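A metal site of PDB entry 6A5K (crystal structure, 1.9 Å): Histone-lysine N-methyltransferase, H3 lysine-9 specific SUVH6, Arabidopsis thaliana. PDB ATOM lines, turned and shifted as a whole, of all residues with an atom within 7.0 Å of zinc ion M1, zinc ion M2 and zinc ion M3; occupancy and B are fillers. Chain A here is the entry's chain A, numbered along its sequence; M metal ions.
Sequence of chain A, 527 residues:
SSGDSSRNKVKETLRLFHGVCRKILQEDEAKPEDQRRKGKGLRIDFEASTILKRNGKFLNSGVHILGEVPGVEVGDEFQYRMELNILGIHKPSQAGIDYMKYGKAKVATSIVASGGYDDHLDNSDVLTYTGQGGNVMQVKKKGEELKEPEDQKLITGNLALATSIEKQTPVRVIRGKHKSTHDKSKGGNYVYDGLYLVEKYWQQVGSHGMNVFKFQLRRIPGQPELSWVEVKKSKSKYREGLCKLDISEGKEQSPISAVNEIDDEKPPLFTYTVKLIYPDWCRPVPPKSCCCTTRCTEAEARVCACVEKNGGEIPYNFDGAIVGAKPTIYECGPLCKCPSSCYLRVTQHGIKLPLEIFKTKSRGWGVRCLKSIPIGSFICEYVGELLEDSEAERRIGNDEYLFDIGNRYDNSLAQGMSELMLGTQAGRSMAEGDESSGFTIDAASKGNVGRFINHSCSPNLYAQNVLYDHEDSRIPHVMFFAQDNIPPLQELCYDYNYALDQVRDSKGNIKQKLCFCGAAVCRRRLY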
ATOM      1  N   LYS A 288      29.349   0.483  35.424  1.00  0.00           N
ATOM      2  CA  LYS A 288      28.192  -0.295  35.009  1.00  0.00           C
ATOM      3  C   LYS A 288      28.618  -1.264  33.914  1.00  0.00           C
ATOM      4  O   LYS A 288      29.339  -0.895  32.989  1.00  0.00           O
ATOM      5  CB  LYS A 288      27.063   0.608  34.519  1.00  0.00           C
ATOM      6  CG  LYS A 288      25.737  -0.112  34.315  1.00  0.00           C
ATOM      7  CD  LYS A 288      24.884   0.559  33.254  1.00  0.00           C
ATOM      8  CE  LYS A 288      23.490  -0.051  33.196  1.00  0.00           C
ATOM      9  NZ  LYS A 288      23.531  -1.534  33.070  1.00  0.00           N
ATOM     10  N   SER A 289      28.174  -2.521  34.016  1.00  0.00           N
ATOM     11  CA  SER A 289      28.551  -3.519  33.022  1.00  0.00           C
ATOM     12  C   SER A 289      27.341  -4.008  32.230  1.00  0.00           C
ATOM     13  O   SER A 289      26.196  -3.756  32.614  1.00  0.00           O
ATOM     14  CB  SER A 289      29.265  -4.686  33.700  1.00  0.00           C
ATOM     15  OG  SER A 289      28.446  -5.247  34.722  1.00  0.00           O
ATOM     16  N   CYS A 290      27.605  -4.703  31.130  1.00  0.00           N
ATOM     17  CA  CYS A 290      26.533  -5.208  30.272  1.00  0.00           C
ATOM     18  C   CYS A 290      26.293  -6.694  30.521  1.00  0.00           C
ATOM     19  O   CYS A 290      27.161  -7.376  31.070  1.00  0.00           O
ATOM     20  CB  CYS A 290      26.852  -4.958  28.792  1.00  0.00           C
ATOM     21  SG  CYS A 290      28.154  -6.011  28.108  1.00  0.00           S
ATOM     22  N   CYS A 291      25.128  -7.191  30.121  1.00  0.00           N
ATOM     23  CA  CYS A 291      24.765  -8.572  30.394  1.00  0.00           C
ATOM     24  C   CYS A 291      24.858  -9.467  29.158  1.00  0.00           C
ATOM     25  O   CYS A 291      24.372 -10.599  29.158  1.00  0.00           O
ATOM     26  CB  CYS A 291      23.350  -8.637  30.973  1.00  0.00           C
ATOM     27  SG  CYS A 291      22.066  -7.842  29.992  1.00  0.00           S
ATOM     28  N   CYS A 292      25.512  -8.974  28.113  1.00  0.00           N
ATOM     29  CA  CYS A 292      25.670  -9.716  26.870  1.00  0.00           C
ATOM     30  C   CYS A 292      26.583 -10.916  27.063  1.00  0.00           C
ATOM     31  O   CYS A 292      27.662 -10.798  27.635  1.00  0.00           O
ATOM     32  CB  CYS A 292      26.227  -8.818  25.776  1.00  0.00           C
ATOM     33  SG  CYS A 292      25.246  -7.332  25.519  1.00  0.00           S
ATOM     34  N   THR A 293      26.160 -12.086  26.580  1.00  0.00           N
ATOM     35  CA  THR A 293      26.982 -13.280  26.702  1.00  0.00           C
ATOM     36  C   THR A 293      27.799 -13.506  25.436  1.00  0.00           C
ATOM     37  O   THR A 293      28.826 -14.183  25.465  1.00  0.00           O
ATOM     38  CB  THR A 293      26.126 -14.540  26.988  1.00  0.00           C
ATOM     39  OG1 THR A 293      25.166 -14.724  25.941  1.00  0.00           O
ATOM     40  CG2 THR A 293      25.398 -14.390  28.304  1.00  0.00           C
ATOM     41  N   THR A 294      27.356 -12.908  24.335  1.00  0.00           N
ATOM     42  CA  THR A 294      28.106 -12.966  23.085  1.00  0.00           C
ATOM     43  C   THR A 294      28.769 -11.613  22.827  1.00  0.00           C
ATOM     44  O   THR A 294      28.628 -10.680  23.634  1.00  0.00           O
ATOM     45  CB  THR A 294      27.206 -13.331  21.878  1.00  0.00           C
ATOM     46  OG1 THR A 294      26.320 -12.254  21.584  1.00  0.00           O
ATOM     47  CG2 THR A 294      26.390 -14.590  22.184  1.00  0.00           C
ATOM     48  N   ARG A 295      29.455 -11.480  21.715  1.00  0.00           N
ATOM     49  CA  ARG A 295      30.099 -10.220  21.363  1.00  0.00           C
ATOM     50  C   ARG A 295      29.058  -9.107  21.147  1.00  0.00           C
ATOM     51  O   ARG A 295      28.090  -9.303  20.470  1.00  0.00           O
ATOM     52  CB  ARG A 295      31.023 -10.460  20.155  1.00  0.00           C
ATOM     53  CG  ARG A 295      32.263 -11.293  20.445  1.00  0.00           C
ATOM     54  CD  ARG A 295      33.101 -11.567  19.204  1.00  0.00           C
ATOM     55  NE  ARG A 295      32.276 -11.958  18.080  1.00  0.00           N
ATOM     56  CZ  ARG A 295      32.765 -12.454  16.950  1.00  0.00           C
ATOM     57  NH1 ARG A 295      31.960 -12.840  15.986  1.00  0.00           N
ATOM     58  NH2 ARG A 295      34.070 -12.563  16.802  1.00  0.00           N
ATOM     59  N   CYS A 296      29.300  -7.913  21.689  1.00  0.00           N
ATOM     60  CA  CYS A 296      28.372  -6.784  21.524  1.00  0.00           C
ATOM     61  C   CYS A 296      28.330  -6.126  20.193  1.00  0.00           C
ATOM     62  O   CYS A 296      29.316  -5.847  19.649  1.00  0.00           O
ATOM     63  CB  CYS A 296      28.622  -5.835  22.750  1.00  0.00           C
ATOM     64  SG  CYS A 296      28.897  -6.607  24.388  1.00  0.00           S
ATOM     65  N   THR A 297      27.127  -5.896  19.733  1.00  0.00           N
ATOM     66  CA  THR A 297      26.821  -5.338  18.430  1.00  0.00           C
ATOM     67  C   THR A 297      25.644  -4.324  18.496  1.00  0.00           C
ATOM     68  O   THR A 297      24.915  -4.323  19.407  1.00  0.00           O
ATOM     69  CB  THR A 297      26.520  -6.485  17.378  1.00  0.00           C
ATOM     70  OG1 THR A 297      25.265  -7.072  17.639  1.00  0.00           O
ATOM     71  CG2 THR A 297      27.594  -7.635  17.271  1.00  0.00           C
ATOM     72  N   VAL A 303      19.455  -3.120  24.499  1.00  0.00           N
ATOM     73  CA  VAL A 303      19.855  -4.433  25.020  1.00  0.00           C
ATOM     74  C   VAL A 303      21.211  -4.361  25.725  1.00  0.00           C
ATOM     75  O   VAL A 303      21.342  -4.810  26.866  1.00  0.00           O
ATOM     76  CB  VAL A 303      19.910  -5.478  23.896  1.00  0.00           C
ATOM     77  CG1 VAL A 303      20.409  -6.817  24.432  1.00  0.00           C
ATOM     78  CG2 VAL A 303      18.536  -5.650  23.247  1.00  0.00           C
ATOM     79  N   CYS A 304      22.203  -3.795  25.049  1.00  0.00           N
ATOM     80  CA  CYS A 304      23.548  -3.686  25.609  1.00  0.00           C
ATOM     81  C   CYS A 304      23.814  -2.291  26.173  1.00  0.00           C
ATOM     82  O   CYS A 304      23.760  -1.299  25.434  1.00  0.00           O
ATOM     83  CB  CYS A 304      24.611  -4.027  24.566  1.00  0.00           C
ATOM     84  SG  CYS A 304      26.304  -3.743  25.143  1.00  0.00           S
ATOM     85  N   ALA A 305      24.109  -2.229  27.464  1.00  0.00           N
ATOM     86  CA  ALA A 305      24.350  -0.962  28.140  1.00  0.00           C
ATOM     87  C   ALA A 305      25.564  -0.234  27.564  1.00  0.00           C
ATOM     88  O   ALA A 305      25.597   0.997  27.498  1.00  0.00           O
ATOM     89  CB  ALA A 305      24.543  -1.190  29.636  1.00  0.00           C
ATOM     90  N   CYS A 306      26.571  -1.003  27.149  1.00  0.00           N
ATOM     91  CA  CYS A 306      27.824  -0.421  26.702  1.00  0.00           C
ATOM     92  C   CYS A 306      27.681   0.162  25.300  1.00  0.00           C
ATOM     93  O   CYS A 306      28.303   1.171  24.978  1.00  0.00           O
ATOM     94  CB  CYS A 306      28.918  -1.475  26.775  1.00  0.00           C
ATOM     95  SG  CYS A 306      29.122  -2.099  28.471  1.00  0.00           S
ATOM     96  N   VAL A 307      26.868  -0.472  24.467  1.00  0.00           N
ATOM     97  CA  VAL A 307      26.518   0.085  23.173  1.00  0.00           C
ATOM     98  C   VAL A 307      25.793   1.411  23.383  1.00  0.00           C
ATOM     99  O   VAL A 307      26.010   2.384  22.654  1.00  0.00           O
ATOM    100  CB  VAL A 307      25.633  -0.872  22.349  1.00  0.00           C
ATOM    101  CG1 VAL A 307      25.070  -0.183  21.108  1.00  0.00           C
ATOM    102  CG2 VAL A 307      26.413  -2.119  21.981  1.00  0.00           C
ATOM    103  N   LYS A 309      26.093   3.436  25.991  1.00  0.00           N
ATOM    104  CA  LYS A 309      27.078   4.437  26.399  1.00  0.00           C
ATOM    105  C   LYS A 309      27.712   5.116  25.184  1.00  0.00           C
ATOM    106  O   LYS A 309      27.978   6.318  25.194  1.00  0.00           O
ATOM    107  CB  LYS A 309      28.187   3.791  27.253  1.00  0.00           C
ATOM    108  CG  LYS A 309      27.752   3.304  28.621  1.00  0.00           C
ATOM    109  CD  LYS A 309      28.973   2.853  29.430  1.00  0.00           C
ATOM    110  CE  LYS A 309      28.601   1.892  30.551  1.00  0.00           C
ATOM    111  NZ  LYS A 309      29.810   1.378  31.259  1.00  0.00           N
ATOM    112  N   GLU A 331      34.631   1.113  26.297  1.00  0.00           N
ATOM    113  CA  GLU A 331      34.841  -0.305  26.065  1.00  0.00           C
ATOM    114  C   GLU A 331      34.158  -1.109  27.161  1.00  0.00           C
ATOM    115  O   GLU A 331      33.862  -0.576  28.231  1.00  0.00           O
ATOM    116  CB  GLU A 331      36.330  -0.636  26.003  1.00  0.00           C
ATOM    117  CG  GLU A 331      37.048  -0.002  24.815  1.00  0.00           C
ATOM    118  CD  GLU A 331      38.434  -0.571  24.593  1.00  0.00           C
ATOM    119  OE1 GLU A 331      38.788  -1.582  25.246  1.00  0.00           O
ATOM    120  OE2 GLU A 331      39.165  -0.019  23.751  1.00  0.00           O
ATOM    121  N   CYS A 332      33.896  -2.378  26.888  1.00  0.00           N
ATOM    122  CA  CYS A 332      33.362  -3.257  27.913  1.00  0.00           C
ATOM    123  C   CYS A 332      34.395  -3.460  29.013  1.00  0.00           C
ATOM    124  O   CYS A 332      35.602  -3.416  28.755  1.00  0.00           O
ATOM    125  CB  CYS A 332      32.913  -4.581  27.308  1.00  0.00           C
ATOM    126  SG  CYS A 332      31.398  -4.405  26.383  1.00  0.00           S
ATOM    127  N   GLY A 333      33.917  -3.652  30.234  1.00  0.00           N
ATOM    128  CA  GLY A 333      34.779  -3.710  31.393  1.00  0.00           C
ATOM    129  C   GLY A 333      34.927  -5.091  31.995  1.00  0.00           C
ATOM    130  O   GLY A 333      34.475  -6.084  31.412  1.00  0.00           O
ATOM    131  N   LEU A 335      33.511  -6.625  34.470  1.00  0.00           N
ATOM    132  CA  LEU A 335      32.327  -7.375  34.887  1.00  0.00           C
ATOM    133  C   LEU A 335      31.309  -7.583  33.761  1.00  0.00           C
ATOM    134  O   LEU A 335      30.235  -8.143  33.997  1.00  0.00           O
ATOM    135  CB  LEU A 335      31.644  -6.665  36.064  1.00  0.00           C
ATOM    136  CG  LEU A 335      32.427  -6.553  37.373  1.00  0.00           C
ATOM    137  CD1 LEU A 335      31.480  -6.295  38.534  1.00  0.00           C
ATOM    138  CD2 LEU A 335      33.264  -7.804  37.612  1.00  0.00           C
ATOM    139  N   CYS A 336      31.638  -7.127  32.549  1.00  0.00           N
ATOM    140  CA  CYS A 336      30.783  -7.379  31.390  1.00  0.00           C
ATOM    141  C   CYS A 336      30.788  -8.878  31.066  1.00  0.00           C
ATOM    142  O   CYS A 336      31.839  -9.505  31.061  1.00  0.00           O
ATOM    143  CB  CYS A 336      31.240  -6.577  30.177  1.00  0.00           C
ATOM    144  SG  CYS A 336      30.888  -4.798  30.232  1.00  0.00           S
ATOM    145  N   LYS A 337      29.608  -9.443  30.794  1.00  0.00           N
ATOM    146  CA  LYS A 337      29.485 -10.885  30.602  1.00  0.00           C
ATOM    147  C   LYS A 337      30.053 -11.333  29.247  1.00  0.00           C
ATOM    148  O   LYS A 337      30.184 -12.524  29.000  1.00  0.00           O
ATOM    149  CB  LYS A 337      28.019 -11.333  30.702  1.00  0.00           C
ATOM    150  CG  LYS A 337      27.285 -10.914  31.969  1.00  0.00           C
ATOM    151  CD  LYS A 337      25.883 -11.513  31.966  1.00  0.00           C
ATOM    152  CE  LYS A 337      25.188 -11.401  33.309  1.00  0.00           C
ATOM    153  NZ  LYS A 337      23.794 -11.951  33.235  1.00  0.00           N
ATOM    154  N   CYS A 338      30.354 -10.369  28.380  1.00  0.00           N
ATOM    155  CA  CYS A 338      30.808 -10.672  27.028  1.00  0.00           C
ATOM    156  C   CYS A 338      32.211 -11.285  27.009  1.00  0.00           C
ATOM    157  O   CYS A 338      33.000 -11.071  27.931  1.00  0.00           O
ATOM    158  CB  CYS A 338      30.783  -9.390  26.189  1.00  0.00           C
ATOM    159  SG  CYS A 338      31.800  -8.091  26.882  1.00  0.00           S
ATOM    160  N   PRO A 339      32.529 -12.057  25.960  1.00  0.00           N
ATOM    161  CA  PRO A 339      33.859 -12.664  25.894  1.00  0.00           C
ATOM    162  C   PRO A 339      34.973 -11.643  25.628  1.00  0.00           C
ATOM    163  O   PRO A 339      34.714 -10.490  25.271  1.00  0.00           O
ATOM    164  CB  PRO A 339      33.739 -13.647  24.723  1.00  0.00           C
ATOM    165  CG  PRO A 339      32.639 -13.081  23.879  1.00  0.00           C
ATOM    166  CD  PRO A 339      31.669 -12.478  24.838  1.00  0.00           C
ATOM    167  N   CYS A 342      35.131  -9.627  22.444  1.00  0.00           N
ATOM    168  CA  CYS A 342      34.096  -8.624  22.216  1.00  0.00           C
ATOM    169  C   CYS A 342      34.621  -7.470  21.371  1.00  0.00           C
ATOM    170  O   CYS A 342      35.727  -6.989  21.591  1.00  0.00           O
ATOM    171  CB  CYS A 342      33.564  -8.065  23.538  1.00  0.00           C
ATOM    172  SG  CYS A 342      32.374  -6.718  23.283  1.00  0.00           S
ATOM    173  N   TYR A 343      33.793  -7.046  20.418  1.00  0.00           N
ATOM    174  CA  TYR A 343      34.179  -5.959  19.518  1.00  0.00           C
ATOM    175  C   TYR A 343      34.457  -4.659  20.278  1.00  0.00           C
ATOM    176  O   TYR A 343      35.172  -3.779  19.793  1.00  0.00           O
ATOM    177  CB  TYR A 343      33.065  -5.749  18.478  1.00  0.00           C
ATOM    178  CG  TYR A 343      32.842  -6.969  17.610  1.00  0.00           C
ATOM    179  CD1 TYR A 343      33.898  -7.582  16.949  1.00  0.00           C
ATOM    180  CD2 TYR A 343      31.571  -7.526  17.469  1.00  0.00           C
ATOM    181  CE1 TYR A 343      33.711  -8.699  16.149  1.00  0.00           C
ATOM    182  CE2 TYR A 343      31.369  -8.644  16.666  1.00  0.00           C
ATOM    183  CZ  TYR A 343      32.445  -9.225  16.014  1.00  0.00           C
ATOM    184  OH  TYR A 343      32.249 -10.322  15.220  1.00  0.00           O
ATOM    185  N   LEU A 344      33.897  -4.564  21.483  1.00  0.00           N
ATOM    186  CA  LEU A 344      34.138  -3.423  22.355  1.00  0.00           C
ATOM    187  C   LEU A 344      35.273  -3.663  23.355  1.00  0.00           C
ATOM    188  O   LEU A 344      35.342  -3.006  24.382  1.00  0.00           O
ATOM    189  CB  LEU A 344      32.864  -3.068  23.118  1.00  0.00           C
ATOM    190  CG  LEU A 344      31.712  -2.514  22.288  1.00  0.00           C
ATOM    191  CD1 LEU A 344      30.526  -2.192  23.201  1.00  0.00           C
ATOM    192  CD2 LEU A 344      32.172  -1.281  21.525  1.00  0.00           C
ATOM    193  N   ARG A 345      36.150  -4.615  23.060  1.00  0.00           N
ATOM    194  CA  ARG A 345      37.368  -4.777  23.857  1.00  0.00           C
ATOM    195  C   ARG A 345      38.574  -4.698  22.933  1.00  0.00           C
ATOM    196  O   ARG A 345      38.900  -5.651  22.239  1.00  0.00           O
ATOM    197  CB  ARG A 345      37.356  -6.111  24.614  1.00  0.00           C
ATOM    198  CG  ARG A 345      36.248  -6.264  25.631  1.00  0.00           C
ATOM    199  CD  ARG A 345      36.396  -7.592  26.367  1.00  0.00           C
ATOM    200  NE  ARG A 345      35.239  -7.942  27.181  1.00  0.00           N
ATOM    201  CZ  ARG A 345      35.108  -7.608  28.463  1.00  0.00           C
ATOM    202  NH1 ARG A 345      36.064  -6.884  29.058  1.00  0.00           N
ATOM    203  NH2 ARG A 345      34.036  -7.977  29.139  1.00  0.00           N
HETATM  204 ZN    ZN M   1      31.088  -6.535  25.304  1.00  0.00          ZN
HETATM  205 ZN    ZN M   2      29.822  -4.288  28.201  1.00  0.00          ZN
HETATM  206 ZN    ZN M   3      27.230  -5.773  25.759  1.00  0.00          ZN
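Of the 28 residues printed, 4 come within 4 Å of zinc ion M1. The nearest printed residue that does not touch zinc ion M1 is Cys 290 (4.1 Å).
Zinc ion M2 is bound by the side-chain sulfur (SG) of Cys 306 (2.3 Å), the side-chain sulfur (SG) of Cys 336 (2.3 Å), the side-chain sulfur (SG) of Cys 290 (2.4 Å) and the side-chain sulfur (SG) of Cys 332 (2.4 Å). Zinc ion M2 has four donor atoms within binding distance.
Zinc ion M1 is bound by the side-chain sulfur of Cys 338 (2.3 Å), the side-chain sulfur of Cys 296 (2.4 Å), the side-chain sulfur of Cys 342 (2.4 Å) and the side-chain sulfur of Cys 332 (2.4 Å).
Along chain A the residues within 4 Å of zinc ion M3 span positions 290 to 304.
The backbone NH (N) of Cys 306 lies close to the side-chain sulfur (SG) of Cys 304 (3.4 Å). The side-chain sulfur (SG) of Cys 304 sits close to the backbone NH (N) of Val 307 (3.4 Å). The backbone NH of Cys 338 is in hydrogen-bond range of the backbone carbonyl oxygen of Cys 292 (2.8 Å). The guanidinium group of Arg 345 sits at hydrogen-bond distance from the backbone carbonyl oxygen of Cys 338, at 3.5 Å. The side-chain sulfur (SG) of Cys 336 lies close to the backbone NH (N) of Gly 333, 3.2 Å away. The backbone carbonyl oxygen of Cys 336 sits close to the guanidinium group of Arg 345, 3.3 Å away. The backbone carbonyl oxygen (O) of Cys 290 sits at hydrogen-bond distance from the backbone NH (N) of Lys 337, at 3.2 Å. N of Leu 344 sits close to SG of Cys 342, at 3.2 Å.
Within 4 Å of zinc ion M2: Cys 290, Cys 306, Cys 332 and Cys 336. The nearest printed residue that does not touch zinc ion M2 is Cys 338 (4.5 Å).
Zinc ion M3 is bound by SG of Cys 296, at 2.3 Å. SG of Cys 304 binds zinc ion M3 (2.3 Å). Zinc ion M3 is bound by SG of Cys 292, at 2.5 Å. Zinc ion M3 is bound by SG of Cys 290, at 2.5 Å.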
